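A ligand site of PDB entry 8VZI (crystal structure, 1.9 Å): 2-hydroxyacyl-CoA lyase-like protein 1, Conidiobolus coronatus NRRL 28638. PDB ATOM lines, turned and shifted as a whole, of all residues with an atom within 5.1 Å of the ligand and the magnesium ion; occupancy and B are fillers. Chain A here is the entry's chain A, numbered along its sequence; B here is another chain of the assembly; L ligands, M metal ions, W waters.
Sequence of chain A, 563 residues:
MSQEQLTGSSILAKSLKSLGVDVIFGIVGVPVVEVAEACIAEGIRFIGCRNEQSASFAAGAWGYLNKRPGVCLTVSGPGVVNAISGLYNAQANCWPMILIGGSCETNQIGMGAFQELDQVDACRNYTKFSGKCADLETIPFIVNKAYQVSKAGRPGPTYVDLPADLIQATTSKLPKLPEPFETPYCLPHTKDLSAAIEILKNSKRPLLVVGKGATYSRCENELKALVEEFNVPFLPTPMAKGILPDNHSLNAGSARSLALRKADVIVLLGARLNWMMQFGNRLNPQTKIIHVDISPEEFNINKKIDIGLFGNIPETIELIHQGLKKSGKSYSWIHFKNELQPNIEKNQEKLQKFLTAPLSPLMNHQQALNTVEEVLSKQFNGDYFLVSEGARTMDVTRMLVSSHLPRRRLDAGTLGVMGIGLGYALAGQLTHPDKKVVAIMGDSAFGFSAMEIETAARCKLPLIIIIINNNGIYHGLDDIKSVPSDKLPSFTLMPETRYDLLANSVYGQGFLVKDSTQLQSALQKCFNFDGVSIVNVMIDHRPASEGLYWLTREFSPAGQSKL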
ATOM      1  N   HIS A 365      28.650   6.849 -26.903  1.00  0.00           N
ATOM      2  CA  HIS A 365      28.355   5.742 -27.805  1.00  0.00           C
ATOM      3  C   HIS A 365      28.780   6.061 -29.248  1.00  0.00           C
ATOM      4  O   HIS A 365      29.454   5.263 -29.902  1.00  0.00           O
ATOM      5  CB  HIS A 365      26.866   5.414 -27.785  1.00  0.00           C
ATOM      6  CG  HIS A 365      26.390   4.680 -26.564  1.00  0.00           C
ATOM      7  ND1 HIS A 365      25.983   5.321 -25.418  1.00  0.00           N
ATOM      8  CD2 HIS A 365      26.169   3.363 -26.350  1.00  0.00           C
ATOM      9  CE1 HIS A 365      25.563   4.437 -24.534  1.00  0.00           C
ATOM     10  NE2 HIS A 365      25.664   3.233 -25.075  1.00  0.00           N
ATOM     11  N   GLU A 389      24.249  -6.234 -30.666  1.00  0.00           N
ATOM     12  CA  GLU A 389      23.293  -6.530 -29.611  1.00  0.00           C
ATOM     13  C   GLU A 389      23.470  -5.559 -28.453  1.00  0.00           C
ATOM     14  O   GLU A 389      24.590  -5.248 -28.063  1.00  0.00           O
ATOM     15  CB  GLU A 389      23.475  -7.966 -29.125  1.00  0.00           C
ATOM     16  CG  GLU A 389      22.612  -8.377 -27.984  1.00  0.00           C
ATOM     17  CD  GLU A 389      23.020  -9.733 -27.447  1.00  0.00           C
ATOM     18  OE1 GLU A 389      24.231  -9.950 -27.218  1.00  0.00           O
ATOM     19  OE2 GLU A 389      22.143 -10.598 -27.290  1.00  0.00           O
ATOM     20  N   GLY A 390      22.364  -5.108 -27.893  1.00  0.00           N
ATOM     21  CA  GLY A 390      22.371  -4.107 -26.857  1.00  0.00           C
ATOM     22  C   GLY A 390      21.152  -3.239 -27.013  1.00  0.00           C
ATOM     23  O   GLY A 390      20.253  -3.544 -27.799  1.00  0.00           O
ATOM     24  N   ALA A 391      21.119  -2.140 -26.261  1.00  0.00           N
ATOM     25  CA  ALA A 391      20.057  -1.158 -26.447  1.00  0.00           C
ATOM     26  C   ALA A 391      20.611   0.054 -27.175  1.00  0.00           C
ATOM     27  O   ALA A 391      20.523   0.141 -28.403  1.00  0.00           O
ATOM     28  CB  ALA A 391      19.429  -0.772 -25.107  1.00  0.00           C
ATOM     29  N   ARG A 392      21.225   0.995 -26.452  1.00  0.00           N
ATOM     30  CA  ARG A 392      21.807   2.143 -27.133  1.00  0.00           C
ATOM     31  C   ARG A 392      22.977   1.725 -28.015  1.00  0.00           C
ATOM     32  O   ARG A 392      23.147   2.245 -29.127  1.00  0.00           O
ATOM     33  CB  ARG A 392      22.206   3.210 -26.120  1.00  0.00           C
ATOM     34  CG  ARG A 392      20.997   3.732 -25.342  1.00  0.00           C
ATOM     35  CD  ARG A 392      21.425   4.682 -24.234  1.00  0.00           C
ATOM     36  NE  ARG A 392      22.091   5.871 -24.758  1.00  0.00           N
ATOM     37  CZ  ARG A 392      22.797   6.701 -24.021  1.00  0.00           C
ATOM     38  NH1 ARG A 392      22.985   6.497 -22.731  1.00  0.00           N
ATOM     39  NH2 ARG A 392      23.342   7.771 -24.592  1.00  0.00           N
ATOM     40  N   THR A 393      23.788   0.760 -27.548  1.00  0.00           N
ATOM     41  CA  THR A 393      24.866   0.238 -28.390  1.00  0.00           C
ATOM     42  C   THR A 393      24.336  -0.283 -29.722  1.00  0.00           C
ATOM     43  O   THR A 393      24.924  -0.017 -30.779  1.00  0.00           O
ATOM     44  CB  THR A 393      25.621  -0.858 -27.633  1.00  0.00           C
ATOM     45  OG1 THR A 393      26.272  -0.292 -26.482  1.00  0.00           O
ATOM     46  CG2 THR A 393      26.690  -1.457 -28.542  1.00  0.00           C
ATOM     47  N   GLY A 416      13.794  -8.426 -29.977  1.00  0.00           N
ATOM     48  CA  GLY A 416      14.675  -7.577 -29.189  1.00  0.00           C
ATOM     49  C   GLY A 416      15.327  -8.322 -28.052  1.00  0.00           C
ATOM     50  O   GLY A 416      15.400  -7.802 -26.923  1.00  0.00           O
ATOM     51  N   VAL A 417      15.784  -9.545 -28.308  1.00  0.00           N
ATOM     52  CA  VAL A 417      16.286 -10.421 -27.262  1.00  0.00           C
ATOM     53  C   VAL A 417      17.765 -10.130 -27.009  1.00  0.00           C
ATOM     54  O   VAL A 417      18.578 -10.090 -27.947  1.00  0.00           O
ATOM     55  CB  VAL A 417      16.081 -11.892 -27.646  1.00  0.00           C
ATOM     56  CG1 VAL A 417      16.520 -12.143 -29.071  1.00  0.00           C
ATOM     57  CG2 VAL A 417      16.823 -12.809 -26.680  1.00  0.00           C
ATOM     58  N   MET A 418      18.109  -9.909 -25.740  1.00  0.00           N
ATOM     59  CA  MET A 418      19.517  -9.919 -25.344  1.00  0.00           C
ATOM     60  C   MET A 418      19.943 -11.358 -25.062  1.00  0.00           C
ATOM     61  O   MET A 418      19.172 -12.159 -24.554  1.00  0.00           O
ATOM     62  CB  MET A 418      19.744  -9.067 -24.096  1.00  0.00           C
ATOM     63  CG  MET A 418      19.341  -7.608 -24.226  1.00  0.00           C
ATOM     64  SD  MET A 418      20.311  -6.722 -25.453  1.00  0.00           S
ATOM     65  CE  MET A 418      19.200  -6.740 -26.861  1.00  0.00           C
ATOM     66  N   GLY A 442      26.646  -4.407 -26.111  1.00  0.00           N
ATOM     67  CA  GLY A 442      26.608  -3.692 -24.855  1.00  0.00           C
ATOM     68  C   GLY A 442      27.106  -4.546 -23.711  1.00  0.00           C
ATOM     69  O   GLY A 442      27.107  -5.773 -23.770  1.00  0.00           O
ATOM     70  N   ASP A 443      27.559  -3.872 -22.635  1.00  0.00           N
ATOM     71  CA  ASP A 443      28.088  -4.616 -21.501  1.00  0.00           C
ATOM     72  C   ASP A 443      27.013  -5.477 -20.849  1.00  0.00           C
ATOM     73  O   ASP A 443      27.267  -6.633 -20.498  1.00  0.00           O
ATOM     74  CB  ASP A 443      28.754  -3.676 -20.468  1.00  0.00           C
ATOM     75  CG  ASP A 443      27.838  -2.568 -19.952  1.00  0.00           C
ATOM     76  OD1 ASP A 443      27.216  -1.867 -20.765  1.00  0.00           O
ATOM     77  OD2 ASP A 443      27.767  -2.389 -18.713  1.00  0.00           O
ATOM     78  N   SER A 444      25.780  -4.960 -20.728  1.00  0.00           N
ATOM     79  CA  SER A 444      24.708  -5.805 -20.202  1.00  0.00           C
ATOM     80  C   SER A 444      24.430  -6.975 -21.136  1.00  0.00           C
ATOM     81  O   SER A 444      24.385  -8.134 -20.701  1.00  0.00           O
ATOM     82  CB  SER A 444      23.438  -4.980 -19.967  1.00  0.00           C
ATOM     83  OG  SER A 444      22.322  -5.833 -19.691  1.00  0.00           O
ATOM     84  N   ALA A 445      24.267  -6.697 -22.428  1.00  0.00           N
ATOM     85  CA  ALA A 445      23.980  -7.756 -23.391  1.00  0.00           C
ATOM     86  C   ALA A 445      25.024  -8.861 -23.327  1.00  0.00           C
ATOM     87  O   ALA A 445      24.698 -10.057 -23.354  1.00  0.00           O
ATOM     88  CB  ALA A 445      23.908  -7.175 -24.800  1.00  0.00           C
ATOM     89  N   PHE A 448      24.871 -11.923 -20.851  1.00  0.00           N
ATOM     90  CA  PHE A 448      23.940 -13.028 -21.035  1.00  0.00           C
ATOM     91  C   PHE A 448      24.636 -14.272 -21.579  1.00  0.00           C
ATOM     92  O   PHE A 448      24.262 -15.389 -21.225  1.00  0.00           O
ATOM     93  CB  PHE A 448      22.800 -12.622 -21.975  1.00  0.00           C
ATOM     94  CG  PHE A 448      21.756 -11.746 -21.333  1.00  0.00           C
ATOM     95  CD1 PHE A 448      21.967 -10.384 -21.203  1.00  0.00           C
ATOM     96  CD2 PHE A 448      20.558 -12.297 -20.878  1.00  0.00           C
ATOM     97  CE1 PHE A 448      21.000  -9.576 -20.623  1.00  0.00           C
ATOM     98  CE2 PHE A 448      19.582 -11.501 -20.307  1.00  0.00           C
ATOM     99  CZ  PHE A 448      19.802 -10.136 -20.179  1.00  0.00           C
ATOM    100  N   ILE A 468      30.839  -2.224 -25.692  1.00  0.00           N
ATOM    101  CA  ILE A 468      30.608  -0.812 -25.396  1.00  0.00           C
ATOM    102  C   ILE A 468      30.069  -0.757 -23.978  1.00  0.00           C
ATOM    103  O   ILE A 468      28.943  -1.180 -23.713  1.00  0.00           O
ATOM    104  CB  ILE A 468      29.638  -0.183 -26.401  1.00  0.00           C
ATOM    105  CG1 ILE A 468      30.109  -0.441 -27.837  1.00  0.00           C
ATOM    106  CG2 ILE A 468      29.483   1.317 -26.142  1.00  0.00           C
ATOM    107  CD1 ILE A 468      31.483   0.215 -28.191  1.00  0.00           C
ATOM    108  N   ASN A 470      29.104   1.045 -20.562  1.00  0.00           N
ATOM    109  CA  ASN A 470      28.684   2.223 -19.806  1.00  0.00           C
ATOM    110  C   ASN A 470      28.256   1.865 -18.387  1.00  0.00           C
ATOM    111  O   ASN A 470      27.543   2.641 -17.743  1.00  0.00           O
ATOM    112  CB  ASN A 470      27.568   2.971 -20.522  1.00  0.00           C
ATOM    113  CG  ASN A 470      26.324   2.119 -20.742  1.00  0.00           C
ATOM    114  OD1 ASN A 470      26.326   0.923 -20.472  1.00  0.00           O
ATOM    115  ND2 ASN A 470      25.278   2.744 -21.270  1.00  0.00           N
ATOM    116  N   ASN A 471      28.676   0.704 -17.888  1.00  0.00           N
ATOM    117  CA  ASN A 471      28.386   0.274 -16.519  1.00  0.00           C
ATOM    118  C   ASN A 471      26.894   0.035 -16.300  1.00  0.00           C
ATOM    119  O   ASN A 471      26.397   0.265 -15.196  1.00  0.00           O
ATOM    120  CB  ASN A 471      28.876   1.279 -15.467  1.00  0.00           C
ATOM    121  CG  ASN A 471      30.356   1.582 -15.592  1.00  0.00           C
ATOM    122  OD1 ASN A 471      31.130   0.778 -16.100  1.00  0.00           O
ATOM    123  ND2 ASN A 471      30.742   2.752 -15.114  1.00  0.00           N
ATOM    124  N   GLY A 472      26.147  -0.412 -17.305  1.00  0.00           N
ATOM    125  CA  GLY A 472      24.795  -0.816 -16.987  1.00  0.00           C
ATOM    126  C   GLY A 472      23.893  -0.895 -18.214  1.00  0.00           C
ATOM    127  O   GLY A 472      24.363  -0.998 -19.352  1.00  0.00           O
ATOM    128  N   ILE A 473      22.597  -0.831 -17.935  1.00  0.00           N
ATOM    129  CA  ILE A 473      21.522  -1.044 -18.898  1.00  0.00           C
ATOM    130  C   ILE A 473      21.028   0.340 -19.343  1.00  0.00           C
ATOM    131  O   ILE A 473      20.338   1.026 -18.589  1.00  0.00           O
ATOM    132  CB  ILE A 473      20.393  -1.873 -18.279  1.00  0.00           C
ATOM    133  CG1 ILE A 473      20.942  -3.200 -17.752  1.00  0.00           C
ATOM    134  CG2 ILE A 473      19.240  -2.107 -19.273  1.00  0.00           C
ATOM    135  CD1 ILE A 473      19.976  -3.950 -16.872  1.00  0.00           C
ATOM    136  N   TYR A 474      21.411   0.751 -20.564  1.00  0.00           N
ATOM    137  CA  TYR A 474      21.184   2.095 -21.107  1.00  0.00           C
ATOM    138  C   TYR A 474      22.118   3.128 -20.498  1.00  0.00           C
ATOM    139  O   TYR A 474      22.542   4.068 -21.169  1.00  0.00           O
ATOM    140  CB  TYR A 474      19.729   2.552 -20.910  1.00  0.00           C
ATOM    141  CG  TYR A 474      18.701   1.836 -21.755  1.00  0.00           C
ATOM    142  CD1 TYR A 474      18.306   0.539 -21.453  1.00  0.00           C
ATOM    143  CD2 TYR A 474      18.105   2.472 -22.846  1.00  0.00           C
ATOM    144  CE1 TYR A 474      17.340  -0.116 -22.228  1.00  0.00           C
ATOM    145  CE2 TYR A 474      17.147   1.830 -23.612  1.00  0.00           C
ATOM    146  CZ  TYR A 474      16.765   0.535 -23.303  1.00  0.00           C
ATOM    147  OH  TYR A 474      15.810  -0.094 -24.079  1.00  0.00           O
ATOM    148  N   HIS A 475      22.428   2.977 -19.210  1.00  0.00           N
ATOM    149  CA  HIS A 475      23.323   3.878 -18.496  1.00  0.00           C
ATOM    150  C   HIS A 475      23.742   3.183 -17.207  1.00  0.00           C
ATOM    151  O   HIS A 475      23.258   2.097 -16.878  1.00  0.00           O
ATOM    152  CB  HIS A 475      22.664   5.239 -18.206  1.00  0.00           C
ATOM    153  CG  HIS A 475      21.454   5.148 -17.326  1.00  0.00           C
ATOM    154  ND1 HIS A 475      21.249   5.968 -16.239  1.00  0.00           N
ATOM    155  CD2 HIS A 475      20.366   4.342 -17.402  1.00  0.00           C
ATOM    156  CE1 HIS A 475      20.093   5.667 -15.668  1.00  0.00           C
ATOM    157  NE2 HIS A 475      19.544   4.676 -16.353  1.00  0.00           N
ATOM    158  N   ILE B  27      16.156  -8.845 -13.981  1.00  0.00           N
ATOM    159  CA  ILE B  27      16.865  -8.024 -14.962  1.00  0.00           C
ATOM    160  C   ILE B  27      15.850  -7.068 -15.576  1.00  0.00           C
ATOM    161  O   ILE B  27      14.754  -7.491 -15.962  1.00  0.00           O
ATOM    162  CB  ILE B  27      17.538  -8.875 -16.053  1.00  0.00           C
ATOM    163  CG1 ILE B  27      18.473  -9.903 -15.431  1.00  0.00           C
ATOM    164  CG2 ILE B  27      18.308  -7.965 -17.046  1.00  0.00           C
ATOM    165  CD1 ILE B  27      19.260 -10.690 -16.426  1.00  0.00           C
ATOM    166  N   VAL B  28      16.199  -5.787 -15.664  1.00  0.00           N
ATOM    167  CA  VAL B  28      15.239  -4.757 -16.015  1.00  0.00           C
ATOM    168  C   VAL B  28      15.371  -4.394 -17.487  1.00  0.00           C
ATOM    169  O   VAL B  28      16.287  -4.829 -18.185  1.00  0.00           O
ATOM    170  CB  VAL B  28      15.374  -3.510 -15.123  1.00  0.00           C
ATOM    171  CG1 VAL B  28      15.140  -3.883 -13.672  1.00  0.00           C
ATOM    172  CG2 VAL B  28      16.750  -2.839 -15.329  1.00  0.00           C
ATOM    173  N   GLY B  29      14.455  -3.561 -17.964  1.00  0.00           N
ATOM    174  CA  GLY B  29      14.431  -3.117 -19.358  1.00  0.00           C
ATOM    175  C   GLY B  29      13.120  -2.424 -19.659  1.00  0.00           C
ATOM    176  O   GLY B  29      12.518  -1.795 -18.791  1.00  0.00           O
ATOM    177  N   VAL B  30      12.666  -2.602 -20.900  1.00  0.00           N
ATOM    178  CA  VAL B  30      11.256  -2.347 -21.231  1.00  0.00           C
ATOM    179  C   VAL B  30      10.437  -3.558 -20.808  1.00  0.00           C
ATOM    180  O   VAL B  30      10.813  -4.701 -21.115  1.00  0.00           O
ATOM    181  CB  VAL B  30      11.097  -2.081 -22.726  1.00  0.00           C
ATOM    182  CG1 VAL B  30       9.640  -2.275 -23.156  1.00  0.00           C
ATOM    183  CG2 VAL B  30      11.589  -0.666 -23.069  1.00  0.00           C
ATOM    184  N   GLU B  52      18.286 -14.299 -16.834  1.00  0.00           N
ATOM    185  CA  GLU B  52      17.102 -14.591 -16.033  1.00  0.00           C
ATOM    186  C   GLU B  52      17.081 -16.020 -15.503  1.00  0.00           C
ATOM    187  O   GLU B  52      16.420 -16.271 -14.485  1.00  0.00           O
ATOM    188  CB  GLU B  52      15.820 -14.331 -16.814  1.00  0.00           C
ATOM    189  CG  GLU B  52      15.574 -12.857 -17.119  1.00  0.00           C
ATOM    190  CD  GLU B  52      16.255 -12.413 -18.421  1.00  0.00           C
ATOM    191  OE1 GLU B  52      16.936 -13.244 -19.059  1.00  0.00           O
ATOM    192  OE2 GLU B  52      16.088 -11.233 -18.787  1.00  0.00           O
ATOM    193  N   VAL B  75      11.539  -8.877 -17.902  1.00  0.00           N
ATOM    194  CA  VAL B  75      10.875  -8.147 -18.984  1.00  0.00           C
ATOM    195  C   VAL B  75       9.954  -9.092 -19.736  1.00  0.00           C
ATOM    196  O   VAL B  75       9.990 -10.315 -19.543  1.00  0.00           O
ATOM    197  CB  VAL B  75      11.892  -7.493 -19.941  1.00  0.00           C
ATOM    198  CG1 VAL B  75      12.918  -6.702 -19.152  1.00  0.00           C
ATOM    199  CG2 VAL B  75      12.545  -8.542 -20.833  1.00  0.00           C
ATOM    200  N   PRO B  78      11.070 -12.680 -24.194  1.00  0.00           N
ATOM    201  CA  PRO B  78      12.220 -13.548 -23.890  1.00  0.00           C
ATOM    202  C   PRO B  78      12.687 -13.451 -22.439  1.00  0.00           C
ATOM    203  O   PRO B  78      13.351 -14.382 -21.965  1.00  0.00           O
ATOM    204  CB  PRO B  78      13.306 -13.042 -24.851  1.00  0.00           C
ATOM    205  CG  PRO B  78      12.967 -11.616 -25.077  1.00  0.00           C
ATOM    206  CD  PRO B  78      11.442 -11.540 -25.041  1.00  0.00           C
ATOM    207  N   GLY B  79      12.371 -12.368 -21.725  1.00  0.00           N
ATOM    208  CA  GLY B  79      12.685 -12.328 -20.305  1.00  0.00           C
ATOM    209  C   GLY B  79      11.932 -13.394 -19.520  1.00  0.00           C
ATOM    210  O   GLY B  79      12.514 -14.165 -18.753  1.00  0.00           O
ATOM    211  N   ASN B  82      13.139 -17.049 -20.645  1.00  0.00           N
ATOM    212  CA  ASN B  82      14.375 -17.425 -19.954  1.00  0.00           C
ATOM    213  C   ASN B  82      14.104 -17.875 -18.509  1.00  0.00           C
ATOM    214  O   ASN B  82      14.753 -18.805 -18.009  1.00  0.00           O
ATOM    215  CB  ASN B  82      15.375 -16.258 -19.954  1.00  0.00           C
ATOM    216  CG  ASN B  82      16.084 -16.090 -21.279  1.00  0.00           C
ATOM    217  OD1 ASN B  82      15.810 -16.814 -22.227  1.00  0.00           O
ATOM    218  ND2 ASN B  82      17.012 -15.120 -21.338  1.00  0.00           N
ATOM    219  N   GLN B 115       7.852  -7.934 -28.125  1.00  0.00           N
ATOM    220  CA  GLN B 115       7.951  -9.014 -27.138  1.00  0.00           C
ATOM    221  C   GLN B 115       6.559  -9.530 -26.766  1.00  0.00           C
ATOM    222  O   GLN B 115       6.292  -9.856 -25.605  1.00  0.00           O
ATOM    223  CB  GLN B 115       8.743  -8.568 -25.896  1.00  0.00           C
ATOM    224  CG  GLN B 115      10.157  -8.094 -26.290  1.00  0.00           C
ATOM    225  CD  GLN B 115      11.097  -7.795 -25.128  1.00  0.00           C
ATOM    226  OE1 GLN B 115      10.670  -7.496 -24.029  1.00  0.00           O
ATOM    227  NE2 GLN B 115      12.405  -7.856 -25.401  1.00  0.00           N
HETATM  228  N1  LIG L   1      16.365  -9.838 -20.959  1.00  0.00           N
HETATM  229  C1  LIG L   1      16.264 -10.276 -22.230  1.00  0.00           C
HETATM  230  C2  LIG L   1      16.415 -11.741 -22.453  1.00  0.00           C
HETATM  231  N2  LIG L   1      16.057  -9.509 -23.295  1.00  0.00           N
HETATM  232  C3  LIG L   1      15.918  -8.174 -23.099  1.00  0.00           C
HETATM  233  N3  LIG L   1      15.685  -7.426 -24.168  1.00  0.00           N
HETATM  234  C4  LIG L   1      15.983  -7.618 -21.784  1.00  0.00           C
HETATM  235  C5  LIG L   1      16.221  -8.525 -20.773  1.00  0.00           C
HETATM  236  C6  LIG L   1      15.889  -6.144 -21.505  1.00  0.00           C
HETATM  237  N4  LIG L   1      16.984  -5.377 -22.140  1.00  0.00           N
HETATM  238  C7  LIG L   1      16.861  -4.705 -23.282  1.00  0.00           C
HETATM  239  S1  LIG L   1      18.290  -3.963 -23.752  1.00  0.00           S
HETATM  240  C8  LIG L   1      19.105  -4.573 -22.360  1.00  0.00           C
HETATM  241  C9  LIG L   1      18.269  -5.309 -21.593  1.00  0.00           C
HETATM  242  C10 LIG L   1      18.606  -6.008 -20.321  1.00  0.00           C
HETATM  243  C11 LIG L   1      20.560  -4.256 -22.117  1.00  0.00           C
HETATM  244  C12 LIG L   1      20.903  -2.829 -22.455  1.00  0.00           C
HETATM  245  O1  LIG L   1      22.262  -2.575 -22.009  1.00  0.00           O
HETATM  246  P1  LIG L   1      23.542  -2.756 -22.915  1.00  0.00           P
HETATM  247  O2  LIG L   1      23.600  -4.064 -23.599  1.00  0.00           O
HETATM  248  O3  LIG L   1      24.679  -2.501 -21.946  1.00  0.00           O
HETATM  249  O4  LIG L   1      23.392  -1.487 -23.805  1.00  0.00           O
HETATM  250  P2  LIG L   1      23.456   0.074 -23.631  1.00  0.00           P
HETATM  251  O5  LIG L   1      23.880   0.359 -22.223  1.00  0.00           O
HETATM  252  O6  LIG L   1      24.532   0.533 -24.699  1.00  0.00           O
HETATM  253  O7  LIG L   1      22.104   0.574 -23.958  1.00  0.00           O
HETATM  254 MG    MG M   1      25.453  -0.782 -21.277  1.00  0.00          MG
HETATM  255  O   HOH W   1      14.832  -2.260 -22.819  1.00  0.00           O
HETATM  256  O   HOH W   2      13.827  -5.124 -24.255  1.00  0.00           O
HETATM  257  O   HOH W   3      26.602  -0.289 -23.028  1.00  0.00           O
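The backbone NH (N) of Asp 443 sits close to an oxygen (O3) of the ligand, 3.3 Å away.
OE2 of Glu 52 of chain B sits at hydrogen-bond distance from N1 of the ligand, 2.6 Å away.
N of Thr 393 sits at hydrogen-bond distance from O6 of the ligand (3.0 Å).
OG1 of Thr 393 sits at hydrogen-bond distance from O6 of the ligand, at 2.6 Å.
An oxygen (O7) of the ligand lies within hydrogen-bond range of the backbone NH (N) of Arg 392.
A nitrogen (N3) of the ligand lies within hydrogen-bond range of the backbone carbonyl oxygen (O) of Gly 416, 2.8 Å away.
A ring nitrogen (NE2) of His 365 is in hydrogen-bond range of an oxygen (O6) of the ligand, at 3.0 Å.
An oxygen (O3) of the ligand lies close to the backbone NH (N) of Ser 444, at 3.0 Å.
N of Ala 445 sits at hydrogen-bond distance from O2 of the ligand, at 3.0 Å.
The backbone NH of Tyr 474 lies close to an oxygen (O7) of the ligand.
The backbone NH (N) of Ala 391 sits at hydrogen-bond distance from an oxygen (O4) of the ligand (3.4 Å).
The backbone NH (N) of Met 418 lies within hydrogen-bond range of a nitrogen (N2) of the ligand (3.2 Å).
Water W3 lies within hydrogen-bond range of the backbone carbonyl oxygen (O) of Ile 468 (2.6 Å), an oxygen (O6) of the ligand (2.8 Å) and the side-chain hydroxyl (OG1) of Thr 393 (3.5 Å).
Water W2 bridges N3 of the ligand (3.0 Å) and NE2 of Gln 115 of chain B (3.3 Å).
Water W1 lies within hydrogen-bond range of the side-chain hydroxyl (OH) of Tyr 474 and the backbone NH (N) of Val 30 of chain B.
Residues that only touch the ligand: Gly 390 (3.5 Å), Gly 442 (3.3 Å), Phe 448 (3.5 Å), Ile 473 (3.5 Å), Ile 27 of chain B (3.8 Å), Val 28 of chain B (3.4 Å), Gly 29 of chain B (3.99 Å), Val 75 of chain B (3.7 Å), Asn 82 of chain B (3.6 Å) and Gln 115 of chain B (3.5 Å).
Hydrophobic or aromatic side chains within 4 Å of the ligand: His 365, Ala 391, Met 418, Ala 445, Phe 448, Ile 473, Ile 27 of chain B and Val 75 of chain B.
The magnesium ion is bound by an oxygen (O3) of the ligand, 2.0 Å away.
The side-chain amide oxygen (OD1) of Asn 470 binds the magnesium ion, at 2.1 Å.
OD1 of Asp 443 is bound to the magnesium ion (2.1 Å).
Water W3 binds the magnesium ion (2.2 Å).
O5 of the ligand binds the magnesium ion, 2.2 Å away.
O of Gly 472 binds the magnesium ion (2.2 Å).
The magnesium ion has six donor atoms within binding distance.
The backbone NH (N) of Asp 443 sits at hydrogen-bond distance from the backbone carbonyl oxygen (O) of Ile 468 (3.2 Å).
N of Asn 471 sits at hydrogen-bond distance from OD2 of Asp 443 (3.3 Å).
OE1 of Glu 52 of chain B is in hydrogen-bond range of ND2 of Asn 82 of chain B, 3.0 Å away.
The guanidinium group of Arg 392 lies within hydrogen-bond range of the backbone carbonyl oxygen of Tyr 474 (2.9 Å).
The backbone carbonyl oxygen (O) of Gly 416 lies within hydrogen-bond range of the side-chain amide nitrogen (NE2) of Gln 115 of chain B, at 3.4 Å.
The backbone NH (N) of Gly 390 is in hydrogen-bond range of the side-chain sulfur (SD) of Met 418, at 3.6 Å.
O of Glu 389 lies within hydrogen-bond range of N of Gly 442 (3.0 Å).
OD1 of Asn 82 of chain B sits close to O of Pro 78 of chain B, 3.5 Å away.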
